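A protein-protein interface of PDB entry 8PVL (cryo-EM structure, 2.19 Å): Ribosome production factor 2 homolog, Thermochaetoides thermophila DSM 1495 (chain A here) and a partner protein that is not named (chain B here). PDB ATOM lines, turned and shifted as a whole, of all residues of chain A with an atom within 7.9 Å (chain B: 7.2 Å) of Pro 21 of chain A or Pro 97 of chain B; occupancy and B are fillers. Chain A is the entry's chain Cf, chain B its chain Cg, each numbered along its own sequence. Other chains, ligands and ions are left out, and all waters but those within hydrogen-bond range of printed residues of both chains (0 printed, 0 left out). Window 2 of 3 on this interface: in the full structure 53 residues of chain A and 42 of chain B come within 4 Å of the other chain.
The backbone carbonyl oxygen of Arg 19 of chain A lies within hydrogen-bond range of the side-chain amino group of Lys 94 of chain B, at 2.7 Å.
O of Lys 22 of chain A lies within hydrogen-bond range of NH2 of Arg 92 of chain B, at 2.8 Å.
The backbone carbonyl oxygen of Ile 23 of chain A lies within hydrogen-bond range of the guanidinium group of Arg 92 of chain B (3.2 Å).
The guanidinium group of Arg 92 of chain B is in salt-bridge range of the side-chain carboxylate of Glu 25 of chain A (3.2 Å).
The side-chain carboxylate (OE2) of Glu 25 of chain A lies within hydrogen-bond range of the backbone NH (N) of Lys 94 of chain B (2.9 Å).
Ala 20 of chain A touches none of the printed residues of chain B.
Printed residues of chain B within 4 Å of Pro 21 of chain A: Pro 95 (3.6 Å) and Pro 97 (3.6 Å).
Of the printed residues of chain B, Glu 25 of chain A touches Arg 92 (3.2 Å) and Lys 94 (2.9 Å).
Printed residues of chain B within 4 Å of Ala 275 of chain A: Val 96 (3.8 Å).
Of the printed residues of chain A, Arg 92 of chain B touches Lys 22 (2.8 Å), Ile 23 (3.2 Å) and Glu 25 (3.2 Å).
Printed residues of chain A within 4 Å of Lys 94 of chain B: Arg 19 (2.7 Å), Glu 25 (2.9 Å) and Tyr 108 (3.3 Å).
Of the printed residues of chain A, Pro 95 of chain B touches Pro 21 (3.6 Å) and Asp 107 (3.7 Å).
Pro 97 of chain B touches three residues of chain A.
The nearest residue of chain A that does not touch Pro 97 of chain B is Ala 275 of chain A (5.5 Å).
Among the printed residues, merely in contact across the chains: Pro 21 of chain A with Pro 95 of chain B (3.6 Å), Pro 21 of chain A with Pro 97 of chain B (3.6 Å), Lys 22 of chain A with Pro 97 of chain B (3.6 Å), Ile 23 of chain A with Pro 97 of chain B (3.8 Å), Asp 107 of chain A with Pro 95 of chain B (3.7 Å), Tyr 108 of chain A with Lys 94 of chain B (3.3 Å) and Ala 275 of chain A with Val 96 of chain B (3.8 Å).
ND2 of Asn 26 of chain A sits close to NZ of Lys 22 of chain A (3.3 Å).
The guanidinium group of Arg 92 of chain B is in hydrogen-bond range of the backbone carbonyl oxygen of Lys 94 of chain B (2.8 Å).
NH2 of Arg 92 of chain B lies within hydrogen-bond range of O of Pro 95 of chain B (3.4 Å).
Of the 14 printed residues of chain A, 8 touch a printed residue of chain B.
Printed residues of chain B that touch a printed residue of chain A: Arg 92, Lys 94, Pro 95, Val 96 and Pro 97.
Hydrophobic or aromatic side chains of chain B that line the printed part of chain A: Pro 95, Val 96 and Pro 97.
Among the printed residues, 12 pairs touch across the chains.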
ATOM      1  N   LEU A  16     -34.450  11.394 -29.092  1.00  0.00           N
ATOM      2  CA  LEU A  16     -33.147  11.092 -28.504  1.00  0.00           C
ATOM      3  C   LEU A  16     -32.557  12.307 -27.797  1.00  0.00           C
ATOM      4  O   LEU A  16     -31.978  12.179 -26.711  1.00  0.00           O
ATOM      5  CB  LEU A  16     -32.190  10.583 -29.581  1.00  0.00           C
ATOM      6  CG  LEU A  16     -31.978   9.071 -29.704  1.00  0.00           C
ATOM      7  CD1 LEU A  16     -31.183   8.547 -28.519  1.00  0.00           C
ATOM      8  CD2 LEU A  16     -33.296   8.324 -29.845  1.00  0.00           C
ATOM      9  N   GLU A  17     -32.695  13.494 -28.395  1.00  0.00           N
ATOM     10  CA  GLU A  17     -32.203  14.709 -27.753  1.00  0.00           C
ATOM     11  C   GLU A  17     -32.997  15.046 -26.497  1.00  0.00           C
ATOM     12  O   GLU A  17     -32.435  15.592 -25.541  1.00  0.00           O
ATOM     13  CB  GLU A  17     -32.243  15.881 -28.731  1.00  0.00           C
ATOM     14  CG  GLU A  17     -31.135  15.860 -29.768  1.00  0.00           C
ATOM     15  CD  GLU A  17     -31.226  17.018 -30.740  1.00  0.00           C
ATOM     16  OE1 GLU A  17     -32.216  17.776 -30.670  1.00  0.00           O
ATOM     17  OE2 GLU A  17     -30.308  17.172 -31.572  1.00  0.00           O
ATOM     18  N   LYS A  18     -34.296  14.742 -26.485  1.00  0.00           N
ATOM     19  CA  LYS A  18     -35.087  14.923 -25.272  1.00  0.00           C
ATOM     20  C   LYS A  18     -34.644  13.963 -24.177  1.00  0.00           C
ATOM     21  O   LYS A  18     -34.630  14.324 -22.995  1.00  0.00           O
ATOM     22  CB  LYS A  18     -36.571  14.736 -25.581  1.00  0.00           C
ATOM     23  CG  LYS A  18     -37.503  15.339 -24.540  1.00  0.00           C
ATOM     24  CD  LYS A  18     -38.974  15.229 -24.937  1.00  0.00           C
ATOM     25  CE  LYS A  18     -39.193  15.424 -26.434  1.00  0.00           C
ATOM     26  NZ  LYS A  18     -39.339  16.861 -26.794  1.00  0.00           N
ATOM     27  N   ARG A  19     -34.282  12.735 -24.548  1.00  0.00           N
ATOM     28  CA  ARG A  19     -33.809  11.767 -23.566  1.00  0.00           C
ATOM     29  C   ARG A  19     -32.343  11.948 -23.191  1.00  0.00           C
ATOM     30  O   ARG A  19     -31.877  11.283 -22.261  1.00  0.00           O
ATOM     31  CB  ARG A  19     -34.033  10.345 -24.081  1.00  0.00           C
ATOM     32  CG  ARG A  19     -35.490   9.932 -24.101  1.00  0.00           C
ATOM     33  CD  ARG A  19     -35.721   8.718 -24.980  1.00  0.00           C
ATOM     34  NE  ARG A  19     -37.113   8.289 -24.937  1.00  0.00           N
ATOM     35  CZ  ARG A  19     -37.546   7.219 -24.286  1.00  0.00           C
ATOM     36  NH1 ARG A  19     -36.718   6.432 -23.620  1.00  0.00           N
ATOM     37  NH2 ARG A  19     -38.845   6.931 -24.303  1.00  0.00           N
ATOM     38  N   ALA A  20     -31.610  12.812 -23.888  1.00  0.00           N
ATOM     39  CA  ALA A  20     -30.196  13.006 -23.599  1.00  0.00           C
ATOM     40  C   ALA A  20     -30.001  13.723 -22.261  1.00  0.00           C
ATOM     41  O   ALA A  20     -30.862  14.497 -21.833  1.00  0.00           O
ATOM     42  CB  ALA A  20     -29.534  13.806 -24.717  1.00  0.00           C
ATOM     43  N   PRO A  21     -28.888  13.459 -21.570  1.00  0.00           N
ATOM     44  CA  PRO A  21     -28.579  14.211 -20.346  1.00  0.00           C
ATOM     45  C   PRO A  21     -28.355  15.689 -20.634  1.00  0.00           C
ATOM     46  O   PRO A  21     -27.791  16.063 -21.665  1.00  0.00           O
ATOM     47  CB  PRO A  21     -27.300  13.542 -19.832  1.00  0.00           C
ATOM     48  CG  PRO A  21     -27.317  12.181 -20.428  1.00  0.00           C
ATOM     49  CD  PRO A  21     -27.952  12.340 -21.775  1.00  0.00           C
ATOM     50  N   LYS A  22     -28.796  16.533 -19.703  1.00  0.00           N
ATOM     51  CA  LYS A  22     -28.777  17.976 -19.876  1.00  0.00           C
ATOM     52  C   LYS A  22     -28.253  18.650 -18.616  1.00  0.00           C
ATOM     53  O   LYS A  22     -28.206  18.052 -17.538  1.00  0.00           O
ATOM     54  CB  LYS A  22     -30.177  18.519 -20.209  1.00  0.00           C
ATOM     55  CG  LYS A  22     -30.716  18.067 -21.555  1.00  0.00           C
ATOM     56  CD  LYS A  22     -32.219  18.248 -21.647  1.00  0.00           C
ATOM     57  CE  LYS A  22     -32.747  17.721 -22.970  1.00  0.00           C
ATOM     58  NZ  LYS A  22     -34.228  17.820 -23.058  1.00  0.00           N
ATOM     59  N   ILE A  23     -27.853  19.914 -18.769  1.00  0.00           N
ATOM     60  CA  ILE A  23     -27.422  20.705 -17.620  1.00  0.00           C
ATOM     61  C   ILE A  23     -28.617  21.052 -16.742  1.00  0.00           C
ATOM     62  O   ILE A  23     -28.619  20.792 -15.533  1.00  0.00           O
ATOM     63  CB  ILE A  23     -26.678  21.968 -18.089  1.00  0.00           C
ATOM     64  CG1 ILE A  23     -25.334  21.593 -18.714  1.00  0.00           C
ATOM     65  CG2 ILE A  23     -26.479  22.935 -16.933  1.00  0.00           C
ATOM     66  CD1 ILE A  23     -24.402  20.873 -17.770  1.00  0.00           C
ATOM     67  N   VAL A  24     -29.649  21.640 -17.335  1.00  0.00           N
ATOM     68  CA  VAL A  24     -30.926  21.860 -16.669  1.00  0.00           C
ATOM     69  C   VAL A  24     -31.836  20.714 -17.084  1.00  0.00           C
ATOM     70  O   VAL A  24     -32.222  20.606 -18.252  1.00  0.00           O
ATOM     71  CB  VAL A  24     -31.532  23.222 -17.030  1.00  0.00           C
ATOM     72  CG1 VAL A  24     -32.899  23.377 -16.385  1.00  0.00           C
ATOM     73  CG2 VAL A  24     -30.605  24.342 -16.597  1.00  0.00           C
ATOM     74  N   GLU A  25     -32.178  19.857 -16.130  1.00  0.00           N
ATOM     75  CA  GLU A  25     -32.864  18.617 -16.441  1.00  0.00           C
ATOM     76  C   GLU A  25     -34.349  18.853 -16.699  1.00  0.00           C
ATOM     77  O   GLU A  25     -34.937  19.846 -16.264  1.00  0.00           O
ATOM     78  CB  GLU A  25     -32.690  17.611 -15.306  1.00  0.00           C
ATOM     79  CG  GLU A  25     -31.309  16.991 -15.242  1.00  0.00           C
ATOM     80  CD  GLU A  25     -31.250  15.805 -14.306  1.00  0.00           C
ATOM     81  OE1 GLU A  25     -31.953  15.823 -13.275  1.00  0.00           O
ATOM     82  OE2 GLU A  25     -30.508  14.847 -14.605  1.00  0.00           O
ATOM     83  N   ASN A  26     -34.948  17.916 -17.427  1.00  0.00           N
ATOM     84  CA  ASN A  26     -36.390  17.901 -17.589  1.00  0.00           C
ATOM     85  C   ASN A  26     -37.055  17.547 -16.260  1.00  0.00           C
ATOM     86  O   ASN A  26     -36.435  16.911 -15.404  1.00  0.00           O
ATOM     87  CB  ASN A  26     -36.793  16.888 -18.658  1.00  0.00           C
ATOM     88  CG  ASN A  26     -36.243  17.230 -20.024  1.00  0.00           C
ATOM     89  OD1 ASN A  26     -36.002  18.395 -20.336  1.00  0.00           O
ATOM     90  ND2 ASN A  26     -36.041  16.211 -20.851  1.00  0.00           N
ATOM     91  N   ASP A 107     -29.721   7.286 -13.855  1.00  0.00           N
ATOM     92  CA  ASP A 107     -29.102   6.718 -15.060  1.00  0.00           C
ATOM     93  C   ASP A 107     -29.677   5.342 -15.394  1.00  0.00           C
ATOM     94  O   ASP A 107     -28.945   4.403 -15.718  1.00  0.00           O
ATOM     95  CB  ASP A 107     -27.578   6.658 -14.926  1.00  0.00           C
ATOM     96  CG  ASP A 107     -26.872   6.707 -16.267  1.00  0.00           C
ATOM     97  OD1 ASP A 107     -27.548   6.944 -17.289  1.00  0.00           O
ATOM     98  OD2 ASP A 107     -25.641   6.505 -16.300  1.00  0.00           O
ATOM     99  N   TYR A 108     -31.007   5.230 -15.287  1.00  0.00           N
ATOM    100  CA  TYR A 108     -31.770   4.006 -15.568  1.00  0.00           C
ATOM    101  C   TYR A 108     -31.338   2.835 -14.687  1.00  0.00           C
ATOM    102  O   TYR A 108     -31.449   1.673 -15.084  1.00  0.00           O
ATOM    103  CB  TYR A 108     -31.696   3.622 -17.050  1.00  0.00           C
ATOM    104  CG  TYR A 108     -31.959   4.778 -17.985  1.00  0.00           C
ATOM    105  CD1 TYR A 108     -33.108   5.549 -17.859  1.00  0.00           C
ATOM    106  CD2 TYR A 108     -31.057   5.104 -18.988  1.00  0.00           C
ATOM    107  CE1 TYR A 108     -33.354   6.607 -18.710  1.00  0.00           C
ATOM    108  CE2 TYR A 108     -31.294   6.161 -19.844  1.00  0.00           C
ATOM    109  CZ  TYR A 108     -32.443   6.909 -19.700  1.00  0.00           C
ATOM    110  OH  TYR A 108     -32.682   7.963 -20.550  1.00  0.00           O
ATOM    111  N   ALA A 275     -24.904  20.818 -11.510  1.00  0.00           N
ATOM    112  CA  ALA A 275     -24.277  21.425 -12.674  1.00  0.00           C
ATOM    113  C   ALA A 275     -24.596  22.912 -12.736  1.00  0.00           C
ATOM    114  O   ALA A 275     -25.695  23.349 -12.383  1.00  0.00           O
ATOM    115  CB  ALA A 275     -24.740  20.739 -13.959  1.00  0.00           C
ATOM    116  N   ARG B  92     -30.410  14.175  -9.109  1.00  0.00           N
ATOM    117  CA  ARG B  92     -30.669  14.229 -10.535  1.00  0.00           C
ATOM    118  C   ARG B  92     -31.183  12.878 -11.023  1.00  0.00           C
ATOM    119  O   ARG B  92     -31.120  11.865 -10.323  1.00  0.00           O
ATOM    120  CB  ARG B  92     -29.404  14.616 -11.298  1.00  0.00           C
ATOM    121  CG  ARG B  92     -28.989  16.062 -11.135  1.00  0.00           C
ATOM    122  CD  ARG B  92     -27.624  16.306 -11.752  1.00  0.00           C
ATOM    123  NE  ARG B  92     -27.581  15.929 -13.158  1.00  0.00           N
ATOM    124  CZ  ARG B  92     -27.786  16.767 -14.164  1.00  0.00           C
ATOM    125  NH1 ARG B  92     -28.045  18.047 -13.956  1.00  0.00           N
ATOM    126  NH2 ARG B  92     -27.729  16.310 -15.411  1.00  0.00           N
ATOM    127  N   LYS B  94     -30.200  11.928 -14.370  1.00  0.00           N
ATOM    128  CA  LYS B  94     -29.125  11.541 -15.264  1.00  0.00           C
ATOM    129  C   LYS B  94     -27.845  12.250 -14.848  1.00  0.00           C
ATOM    130  O   LYS B  94     -27.899  13.327 -14.244  1.00  0.00           O
ATOM    131  CB  LYS B  94     -29.476  11.888 -16.718  1.00  0.00           C
ATOM    132  CG  LYS B  94     -30.552  10.991 -17.303  1.00  0.00           C
ATOM    133  CD  LYS B  94     -31.245  11.635 -18.488  1.00  0.00           C
ATOM    134  CE  LYS B  94     -32.471  10.837 -18.892  1.00  0.00           C
ATOM    135  NZ  LYS B  94     -33.281  11.537 -19.923  1.00  0.00           N
ATOM    136  N   PRO B  95     -26.682  11.661 -15.131  1.00  0.00           N
ATOM    137  CA  PRO B  95     -25.419  12.314 -14.767  1.00  0.00           C
ATOM    138  C   PRO B  95     -25.196  13.603 -15.541  1.00  0.00           C
ATOM    139  O   PRO B  95     -25.750  13.811 -16.623  1.00  0.00           O
ATOM    140  CB  PRO B  95     -24.356  11.265 -15.122  1.00  0.00           C
ATOM    141  CG  PRO B  95     -25.037  10.303 -16.032  1.00  0.00           C
ATOM    142  CD  PRO B  95     -26.464  10.282 -15.600  1.00  0.00           C
ATOM    143  N   VAL B  96     -24.397  14.483 -14.942  1.00  0.00           N
ATOM    144  CA  VAL B  96     -24.044  15.770 -15.553  1.00  0.00           C
ATOM    145  C   VAL B  96     -23.305  15.513 -16.861  1.00  0.00           C
ATOM    146  O   VAL B  96     -22.412  14.642 -16.899  1.00  0.00           O
ATOM    147  CB  VAL B  96     -23.184  16.601 -14.581  1.00  0.00           C
ATOM    148  CG1 VAL B  96     -22.575  17.812 -15.269  1.00  0.00           C
ATOM    149  CG2 VAL B  96     -24.012  17.030 -13.382  1.00  0.00           C
ATOM    150  N   PRO B  97     -23.667  16.185 -17.959  1.00  0.00           N
ATOM    151  CA  PRO B  97     -23.018  15.908 -19.248  1.00  0.00           C
ATOM    152  C   PRO B  97     -21.531  16.227 -19.227  1.00  0.00           C
ATOM    153  O   PRO B  97     -21.089  17.202 -18.615  1.00  0.00           O
ATOM    154  CB  PRO B  97     -23.772  16.816 -20.225  1.00  0.00           C
ATOM    155  CG  PRO B  97     -25.070  17.105 -19.561  1.00  0.00           C
ATOM    156  CD  PRO B  97     -24.777  17.141 -18.096  1.00  0.00           C
ATOM    157  N   GLN B  98     -20.761  15.387 -19.910  1.00  0.00           N
ATOM    158  CA  GLN B  98     -19.318  15.487 -19.973  1.00  0.00           C
ATOM    159  C   GLN B  98     -18.880  15.687 -21.418  1.00  0.00           C
ATOM    160  O   GLN B  98     -19.609  15.311 -22.342  1.00  0.00           O
ATOM    161  CB  GLN B  98     -18.659  14.220 -19.401  1.00  0.00           C
ATOM    162  CG  GLN B  98     -18.749  13.980 -17.866  1.00  0.00           C
ATOM    163  CD  GLN B  98     -18.169  15.077 -16.955  1.00  0.00           C
ATOM    164  OE1 GLN B  98     -18.440  16.271 -17.098  1.00  0.00           O
ATOM    165  NE2 GLN B  98     -17.356  14.648 -15.998  1.00  0.00           N
ATOM    166  N   PRO B  99     -17.721  16.309 -21.648  1.00  0.00           N
ATOM    167  CA  PRO B  99     -17.220  16.438 -23.022  1.00  0.00           C
ATOM    168  C   PRO B  99     -16.922  15.081 -23.642  1.00  0.00           C
ATOM    169  O   PRO B  99     -16.472  14.151 -22.968  1.00  0.00           O
ATOM    170  CB  PRO B  99     -15.946  17.273 -22.856  1.00  0.00           C
ATOM    171  CG  PRO B  99     -16.154  18.025 -21.590  1.00  0.00           C
ATOM    172  CD  PRO B  99     -16.916  17.095 -20.697  1.00  0.00           C
